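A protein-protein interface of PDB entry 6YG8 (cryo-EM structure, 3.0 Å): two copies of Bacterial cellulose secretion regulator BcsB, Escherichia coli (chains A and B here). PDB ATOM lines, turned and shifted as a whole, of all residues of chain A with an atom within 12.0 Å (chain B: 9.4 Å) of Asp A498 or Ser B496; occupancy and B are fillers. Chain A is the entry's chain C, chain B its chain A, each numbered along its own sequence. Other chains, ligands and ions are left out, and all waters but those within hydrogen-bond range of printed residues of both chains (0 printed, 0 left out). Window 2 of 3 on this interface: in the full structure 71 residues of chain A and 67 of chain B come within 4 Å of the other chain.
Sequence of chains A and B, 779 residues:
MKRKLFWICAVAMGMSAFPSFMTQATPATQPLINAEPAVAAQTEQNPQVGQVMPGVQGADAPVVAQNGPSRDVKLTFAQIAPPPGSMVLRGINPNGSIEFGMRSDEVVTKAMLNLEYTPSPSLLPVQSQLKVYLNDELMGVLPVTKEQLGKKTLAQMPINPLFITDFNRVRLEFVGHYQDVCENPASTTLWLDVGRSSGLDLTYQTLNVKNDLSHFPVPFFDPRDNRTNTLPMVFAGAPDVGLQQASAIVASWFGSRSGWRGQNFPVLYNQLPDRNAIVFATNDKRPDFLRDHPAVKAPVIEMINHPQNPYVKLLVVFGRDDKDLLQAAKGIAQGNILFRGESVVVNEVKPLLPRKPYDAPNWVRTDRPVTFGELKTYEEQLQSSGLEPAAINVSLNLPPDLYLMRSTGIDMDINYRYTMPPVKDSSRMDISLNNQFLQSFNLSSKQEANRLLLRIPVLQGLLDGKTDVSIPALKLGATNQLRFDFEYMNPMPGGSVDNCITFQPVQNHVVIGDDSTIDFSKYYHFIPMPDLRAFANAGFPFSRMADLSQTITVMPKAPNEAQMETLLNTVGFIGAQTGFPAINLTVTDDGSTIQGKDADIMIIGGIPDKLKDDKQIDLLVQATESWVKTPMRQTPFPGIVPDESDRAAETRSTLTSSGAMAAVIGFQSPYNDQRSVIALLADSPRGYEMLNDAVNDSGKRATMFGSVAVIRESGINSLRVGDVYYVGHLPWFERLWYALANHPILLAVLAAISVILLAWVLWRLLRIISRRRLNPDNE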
ATOM      1  N   GLN A 179     -23.314 -28.124  21.598  1.00  0.00           N
ATOM      2  CA  GLN A 179     -23.254 -26.784  21.035  1.00  0.00           C
ATOM      3  C   GLN A 179     -24.510 -26.543  20.213  1.00  0.00           C
ATOM      4  O   GLN A 179     -25.073 -27.473  19.633  1.00  0.00           O
ATOM      5  CB  GLN A 179     -21.999 -26.611  20.176  1.00  0.00           C
ATOM      6  CG  GLN A 179     -21.736 -25.202  19.707  1.00  0.00           C
ATOM      7  CD  GLN A 179     -20.461 -25.103  18.901  1.00  0.00           C
ATOM      8  OE1 GLN A 179     -19.801 -26.107  18.641  1.00  0.00           O
ATOM      9  NE2 GLN A 179     -20.105 -23.889  18.504  1.00  0.00           N
ATOM     10  N   ASP A 180     -24.937 -25.280  20.164  1.00  0.00           N
ATOM     11  CA  ASP A 180     -26.179 -24.942  19.474  1.00  0.00           C
ATOM     12  C   ASP A 180     -26.011 -25.029  17.961  1.00  0.00           C
ATOM     13  O   ASP A 180     -26.691 -25.815  17.292  1.00  0.00           O
ATOM     14  CB  ASP A 180     -26.642 -23.547  19.892  1.00  0.00           C
ATOM     15  CG  ASP A 180     -26.718 -23.389  21.395  1.00  0.00           C
ATOM     16  OD1 ASP A 180     -25.661 -23.181  22.025  1.00  0.00           O
ATOM     17  OD2 ASP A 180     -27.833 -23.483  21.947  1.00  0.00           O
ATOM     18  N   VAL A 181     -25.109 -24.226  17.405  1.00  0.00           N
ATOM     19  CA  VAL A 181     -24.849 -24.205  15.974  1.00  0.00           C
ATOM     20  C   VAL A 181     -23.478 -24.808  15.722  1.00  0.00           C
ATOM     21  O   VAL A 181     -22.607 -24.812  16.599  1.00  0.00           O
ATOM     22  CB  VAL A 181     -24.936 -22.775  15.393  1.00  0.00           C
ATOM     23  CG1 VAL A 181     -26.215 -22.097  15.855  1.00  0.00           C
ATOM     24  CG2 VAL A 181     -23.718 -21.962  15.799  1.00  0.00           C
ATOM     25  N   CYS A 182     -23.291 -25.325  14.506  1.00  0.00           N
ATOM     26  CA  CYS A 182     -22.047 -25.978  14.105  1.00  0.00           C
ATOM     27  C   CYS A 182     -21.688 -27.100  15.077  1.00  0.00           C
ATOM     28  O   CYS A 182     -20.669 -27.070  15.768  1.00  0.00           O
ATOM     29  CB  CYS A 182     -20.910 -24.956  13.977  1.00  0.00           C
ATOM     30  SG  CYS A 182     -21.404 -23.409  13.189  1.00  0.00           S
ATOM     31  N   GLU A 183     -22.565 -28.095  15.129  1.00  0.00           N
ATOM     32  CA  GLU A 183     -22.445 -29.207  16.067  1.00  0.00           C
ATOM     33  C   GLU A 183     -22.106 -30.464  15.280  1.00  0.00           C
ATOM     34  O   GLU A 183     -22.993 -31.121  14.727  1.00  0.00           O
ATOM     35  CB  GLU A 183     -23.735 -29.383  16.862  1.00  0.00           C
ATOM     36  CG  GLU A 183     -23.702 -30.533  17.848  1.00  0.00           C
ATOM     37  CD  GLU A 183     -24.740 -30.394  18.937  1.00  0.00           C
ATOM     38  OE1 GLU A 183     -25.940 -30.569  18.639  1.00  0.00           O
ATOM     39  OE2 GLU A 183     -24.355 -30.097  20.087  1.00  0.00           O
ATOM     40  N   ASN A 184     -20.821 -30.797  15.233  1.00  0.00           N
ATOM     41  CA  ASN A 184     -20.372 -32.015  14.578  1.00  0.00           C
ATOM     42  C   ASN A 184     -20.945 -33.221  15.309  1.00  0.00           C
ATOM     43  O   ASN A 184     -20.549 -33.502  16.447  1.00  0.00           O
ATOM     44  CB  ASN A 184     -18.845 -32.078  14.547  1.00  0.00           C
ATOM     45  CG  ASN A 184     -18.327 -33.321  13.855  1.00  0.00           C
ATOM     46  OD1 ASN A 184     -19.067 -34.019  13.166  1.00  0.00           O
ATOM     47  ND2 ASN A 184     -17.042 -33.601  14.032  1.00  0.00           N
ATOM     48  N   GLY A 494     -18.955 -30.531   6.481  1.00  0.00           N
ATOM     49  CA  GLY A 494     -18.970 -29.556   7.552  1.00  0.00           C
ATOM     50  C   GLY A 494     -19.236 -28.143   7.077  1.00  0.00           C
ATOM     51  O   GLY A 494     -19.709 -27.301   7.846  1.00  0.00           O
ATOM     52  N   GLY A 495     -18.938 -27.873   5.811  1.00  0.00           N
ATOM     53  CA  GLY A 495     -19.080 -26.535   5.272  1.00  0.00           C
ATOM     54  C   GLY A 495     -17.771 -25.778   5.282  1.00  0.00           C
ATOM     55  O   GLY A 495     -16.701 -26.386   5.203  1.00  0.00           O
ATOM     56  N   SER A 496     -17.836 -24.458   5.374  1.00  0.00           N
ATOM     57  CA  SER A 496     -16.644 -23.633   5.459  1.00  0.00           C
ATOM     58  C   SER A 496     -16.520 -23.054   6.866  1.00  0.00           C
ATOM     59  O   SER A 496     -17.278 -23.404   7.776  1.00  0.00           O
ATOM     60  CB  SER A 496     -16.679 -22.540   4.392  1.00  0.00           C
ATOM     61  OG  SER A 496     -15.547 -21.696   4.504  1.00  0.00           O
ATOM     62  N   VAL A 497     -15.544 -22.165   7.055  1.00  0.00           N
ATOM     63  CA  VAL A 497     -15.337 -21.564   8.368  1.00  0.00           C
ATOM     64  C   VAL A 497     -16.510 -20.666   8.742  1.00  0.00           C
ATOM     65  O   VAL A 497     -16.974 -20.675   9.888  1.00  0.00           O
ATOM     66  CB  VAL A 497     -14.005 -20.791   8.398  1.00  0.00           C
ATOM     67  CG1 VAL A 497     -13.815 -20.121   9.750  1.00  0.00           C
ATOM     68  CG2 VAL A 497     -12.844 -21.723   8.085  1.00  0.00           C
ATOM     69  N   ASP A 498     -17.015 -19.889   7.786  1.00  0.00           N
ATOM     70  CA  ASP A 498     -18.073 -18.934   8.093  1.00  0.00           C
ATOM     71  C   ASP A 498     -19.439 -19.595   8.193  1.00  0.00           C
ATOM     72  O   ASP A 498     -20.290 -19.128   8.957  1.00  0.00           O
ATOM     73  CB  ASP A 498     -18.106 -17.831   7.037  1.00  0.00           C
ATOM     74  CG  ASP A 498     -18.486 -18.350   5.664  1.00  0.00           C
ATOM     75  OD1 ASP A 498     -19.698 -18.477   5.387  1.00  0.00           O
ATOM     76  OD2 ASP A 498     -17.574 -18.636   4.861  1.00  0.00           O
ATOM     77  N   ASN A 499     -19.674 -20.665   7.441  1.00  0.00           N
ATOM     78  CA  ASN A 499     -20.965 -21.336   7.413  1.00  0.00           C
ATOM     79  C   ASN A 499     -20.782 -22.812   7.731  1.00  0.00           C
ATOM     80  O   ASN A 499     -19.927 -23.477   7.137  1.00  0.00           O
ATOM     81  CB  ASN A 499     -21.640 -21.167   6.051  1.00  0.00           C
ATOM     82  CG  ASN A 499     -23.118 -21.486   6.090  1.00  0.00           C
ATOM     83  OD1 ASN A 499     -23.513 -22.651   6.119  1.00  0.00           O
ATOM     84  ND2 ASN A 499     -23.946 -20.449   6.091  1.00  0.00           N
ATOM     85  N   CYS A 500     -21.587 -23.318   8.661  1.00  0.00           N
ATOM     86  CA  CYS A 500     -21.576 -24.720   9.047  1.00  0.00           C
ATOM     87  C   CYS A 500     -22.898 -25.365   8.663  1.00  0.00           C
ATOM     88  O   CYS A 500     -23.951 -24.721   8.677  1.00  0.00           O
ATOM     89  CB  CYS A 500     -21.330 -24.886  10.551  1.00  0.00           C
ATOM     90  SG  CYS A 500     -22.510 -24.010  11.595  1.00  0.00           S
ATOM     91  N   ILE A 501     -22.836 -26.649   8.328  1.00  0.00           N
ATOM     92  CA  ILE A 501     -23.954 -27.367   7.732  1.00  0.00           C
ATOM     93  C   ILE A 501     -24.509 -28.350   8.748  1.00  0.00           C
ATOM     94  O   ILE A 501     -23.771 -29.186   9.282  1.00  0.00           O
ATOM     95  CB  ILE A 501     -23.526 -28.094   6.449  1.00  0.00           C
ATOM     96  CG1 ILE A 501     -22.683 -27.164   5.578  1.00  0.00           C
ATOM     97  CG2 ILE A 501     -24.742 -28.575   5.692  1.00  0.00           C
ATOM     98  CD1 ILE A 501     -23.415 -25.914   5.128  1.00  0.00           C
ATOM     99  N   THR A 502     -25.808 -28.253   9.005  1.00  0.00           N
ATOM    100  CA  THR A 502     -26.519 -29.196   9.853  1.00  0.00           C
ATOM    101  C   THR A 502     -27.209 -30.225   8.970  1.00  0.00           C
ATOM    102  O   THR A 502     -27.860 -29.866   7.985  1.00  0.00           O
ATOM    103  CB  THR A 502     -27.546 -28.484  10.729  1.00  0.00           C
ATOM    104  OG1 THR A 502     -26.928 -27.376  11.391  1.00  0.00           O
ATOM    105  CG2 THR A 502     -28.097 -29.438  11.760  1.00  0.00           C
ATOM    106  N   CYS B 182     -31.945 -20.095  16.910  1.00  0.00           N
ATOM    107  CA  CYS B 182     -31.002 -21.116  16.455  1.00  0.00           C
ATOM    108  C   CYS B 182     -31.533 -22.516  16.755  1.00  0.00           C
ATOM    109  O   CYS B 182     -30.802 -23.396  17.212  1.00  0.00           O
ATOM    110  CB  CYS B 182     -29.619 -20.918  17.080  1.00  0.00           C
ATOM    111  SG  CYS B 182     -28.862 -19.298  16.827  1.00  0.00           S
ATOM    112  N   PRO B 493     -28.192 -25.305   6.326  1.00  0.00           N
ATOM    113  CA  PRO B 493     -27.154 -24.426   6.868  1.00  0.00           C
ATOM    114  C   PRO B 493     -27.538 -23.876   8.229  1.00  0.00           C
ATOM    115  O   PRO B 493     -28.699 -23.554   8.494  1.00  0.00           O
ATOM    116  CB  PRO B 493     -27.053 -23.305   5.824  1.00  0.00           C
ATOM    117  CG  PRO B 493     -27.671 -23.872   4.587  1.00  0.00           C
ATOM    118  CD  PRO B 493     -28.743 -24.796   5.062  1.00  0.00           C
ATOM    119  N   GLY B 494     -26.545 -23.794   9.106  1.00  0.00           N
ATOM    120  CA  GLY B 494     -26.747 -23.198  10.409  1.00  0.00           C
ATOM    121  C   GLY B 494     -26.241 -21.774  10.480  1.00  0.00           C
ATOM    122  O   GLY B 494     -26.947 -20.883  10.957  1.00  0.00           O
ATOM    123  N   GLY B 495     -25.026 -21.549   9.991  1.00  0.00           N
ATOM    124  CA  GLY B 495     -24.392 -20.250  10.095  1.00  0.00           C
ATOM    125  C   GLY B 495     -23.051 -20.330  10.794  1.00  0.00           C
ATOM    126  O   GLY B 495     -22.195 -21.131  10.413  1.00  0.00           O
ATOM    127  N   SER B 496     -22.850 -19.501  11.812  1.00  0.00           N
ATOM    128  CA  SER B 496     -21.673 -19.580  12.663  1.00  0.00           C
ATOM    129  C   SER B 496     -22.083 -19.309  14.103  1.00  0.00           C
ATOM    130  O   SER B 496     -23.254 -19.058  14.402  1.00  0.00           O
ATOM    131  CB  SER B 496     -20.586 -18.594  12.222  1.00  0.00           C
ATOM    132  OG  SER B 496     -20.906 -17.277  12.630  1.00  0.00           O
ATOM    133  N   VAL B 497     -21.100 -19.363  15.003  1.00  0.00           N
ATOM    134  CA  VAL B 497     -21.380 -19.131  16.417  1.00  0.00           C
ATOM    135  C   VAL B 497     -21.888 -17.713  16.635  1.00  0.00           C
ATOM    136  O   VAL B 497     -22.651 -17.448  17.571  1.00  0.00           O
ATOM    137  CB  VAL B 497     -20.132 -19.428  17.266  1.00  0.00           C
ATOM    138  CG1 VAL B 497     -19.704 -20.872  17.078  1.00  0.00           C
ATOM    139  CG2 VAL B 497     -18.997 -18.484  16.899  1.00  0.00           C
ATOM    140  N   ASP B 498     -21.479 -16.781  15.773  1.00  0.00           N
ATOM    141  CA  ASP B 498     -21.943 -15.405  15.900  1.00  0.00           C
ATOM    142  C   ASP B 498     -23.388 -15.265  15.440  1.00  0.00           C
ATOM    143  O   ASP B 498     -24.221 -14.691  16.150  1.00  0.00           O
ATOM    144  CB  ASP B 498     -21.034 -14.471  15.103  1.00  0.00           C
ATOM    145  CG  ASP B 498     -19.651 -14.346  15.710  1.00  0.00           C
ATOM    146  OD1 ASP B 498     -19.531 -14.480  16.946  1.00  0.00           O
ATOM    147  OD2 ASP B 498     -18.684 -14.116  14.952  1.00  0.00           O
ATOM    148  N   ASN B 499     -23.706 -15.793  14.262  1.00  0.00           N
ATOM    149  CA  ASN B 499     -25.015 -15.616  13.657  1.00  0.00           C
ATOM    150  C   ASN B 499     -25.529 -16.946  13.130  1.00  0.00           C
ATOM    151  O   ASN B 499     -24.778 -17.720  12.530  1.00  0.00           O
ATOM    152  CB  ASN B 499     -24.959 -14.587  12.522  1.00  0.00           C
ATOM    153  CG  ASN B 499     -26.332 -14.179  12.037  1.00  0.00           C
ATOM    154  OD1 ASN B 499     -27.345 -14.512  12.650  1.00  0.00           O
ATOM    155  ND2 ASN B 499     -26.375 -13.451  10.928  1.00  0.00           N
ATOM    156  N   CYS B 500     -26.812 -17.203  13.357  1.00  0.00           N
ATOM    157  CA  CYS B 500     -27.465 -18.393  12.842  1.00  0.00           C
ATOM    158  C   CYS B 500     -28.673 -17.957  12.027  1.00  0.00           C
ATOM    159  O   CYS B 500     -29.037 -16.780  12.009  1.00  0.00           O
ATOM    160  CB  CYS B 500     -27.878 -19.342  13.971  1.00  0.00           C
ATOM    161  SG  CYS B 500     -29.321 -18.807  14.913  1.00  0.00           S
ATOM    162  N   ILE B 501     -29.305 -18.913  11.352  1.00  0.00           N
ATOM    163  CA  ILE B 501     -30.424 -18.623  10.462  1.00  0.00           C
ATOM    164  C   ILE B 501     -31.634 -19.444  10.890  1.00  0.00           C
ATOM    165  O   ILE B 501     -31.493 -20.572  11.375  1.00  0.00           O
ATOM    166  CB  ILE B 501     -30.073 -18.902   8.986  1.00  0.00           C
ATOM    167  CG1 ILE B 501     -29.817 -20.389   8.757  1.00  0.00           C
ATOM    168  CG2 ILE B 501     -28.856 -18.095   8.556  1.00  0.00           C
ATOM    169  CD1 ILE B 501     -29.734 -20.773   7.291  1.00  0.00           C
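O of Gly B495 lies close to O of Asp A498, at 3.1 Å.
The backbone NH (N) of Gly B494 lies within hydrogen-bond range of the backbone carbonyl oxygen (O) of Cys A500.
The side-chain sulfur of Cys A182 sits close to the backbone carbonyl oxygen of Gly B495, at 3.7 Å.
O of Gly B495 is in hydrogen-bond range of N of Cys A500 (2.9 Å).
The side-chain carboxylate (OE2) of Glu A183 sits at hydrogen-bond distance from the backbone NH (N) of Gln A179, at 2.7 Å.
The side-chain sulfur (SG) of Cys B182 forms a disulfide with the side-chain sulfur (SG) of Cys B500.
The side-chain amide oxygen of Gln A179 lies close to the backbone carbonyl oxygen of Cys A182.
The side-chain hydroxyl (OG) of Ser B496 lies close to the backbone NH (N) of Asp B498 (3.2 Å).
O of Val A181 sits close to NE2 of Gln A179 (3.3 Å).
The backbone carbonyl oxygen of Gly B494 lies within hydrogen-bond range of the backbone NH of Ile B501.
NE2 of Gln A179 touches CG1 of Val B497, 3.4 Å away.
Val A181 touches Cys B182.
Ser B496 touches Val A181.
Val A181 touches Val B497 (CG2 to CA, 3.7 Å).
Val A181 touches Cys B500 (CG1 to CB, 3.7 Å).
Cys A182 touches Ser B496 (SG to CA, 3.9 Å).
Asp A498 touches Ser B496.
OD1 of Asn A499 touches CB of Pro B493, at 3.6 Å.
O of Gly B495 touches CA of Asn A499, 3.2 Å away.
Cys A500 touches Pro B493.
Asp A498 touches just these residues of chain B: Gly B495 (3.1 Å) and Ser B496 (3.3 Å).
Ser B496 touches three residues of chain A.
No residue of chain B comes within 4 Å of Ser A496.
No residue of chain B comes within 4 Å of Val A497.
Of chain A, only Cys A500 comes within 4 Å of Gly B494.
No residue of chain A comes within 4 Å of Asp B498.
Printed residues of chain B within 4 Å of Val A181: Cys B182, Ser B496, Val B497 and Cys B500.
Printed residues of chain B within 4 Å of Cys A182: Gly B495 and Ser B496.
Of the printed residues of chain A, Cys B182 touches Val A181.
Printed residues of chain B within 4 Å of Asn A499: Pro B493 (3.6 Å) and Gly B495 (3.2 Å).
Glu A183 touches none of the printed residues of chain B.
Of the 15 printed residues of chain A, 6 touch a printed residue of chain B.
Printed residues of chain A that touch a printed residue of chain B: Gln A179, Val A181, Cys A182, Asp A498, Asn A499 and Cys A500.
Hydrophobic or aromatic side chains of chain A within 4 Å of the printed part of chain B: Val A181.
Cys A182 touches Ser B496, but with the chains exchanged Ser A496 does not touch Cys B182 (15.3 Å).
Asp A498 touches Gly B495, but with the chains exchanged Gly A495 does not touch Asp B498 (14.3 Å).
Asp A498 touches Ser B496, but with the chains exchanged Ser A496 does not touch Asp B498 (11.2 Å).
Cys A500 touches Gly B495, but with the chains exchanged Gly A495 does not touch Cys B500 (13.9 Å).
Positions printed for both chains: 182, 494, 495, 496, 497, 498, 499, 500 and 501.
Of the 14 pairs that touch across the chains among the printed residues, none has its exchanged pair printed and touching as well.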
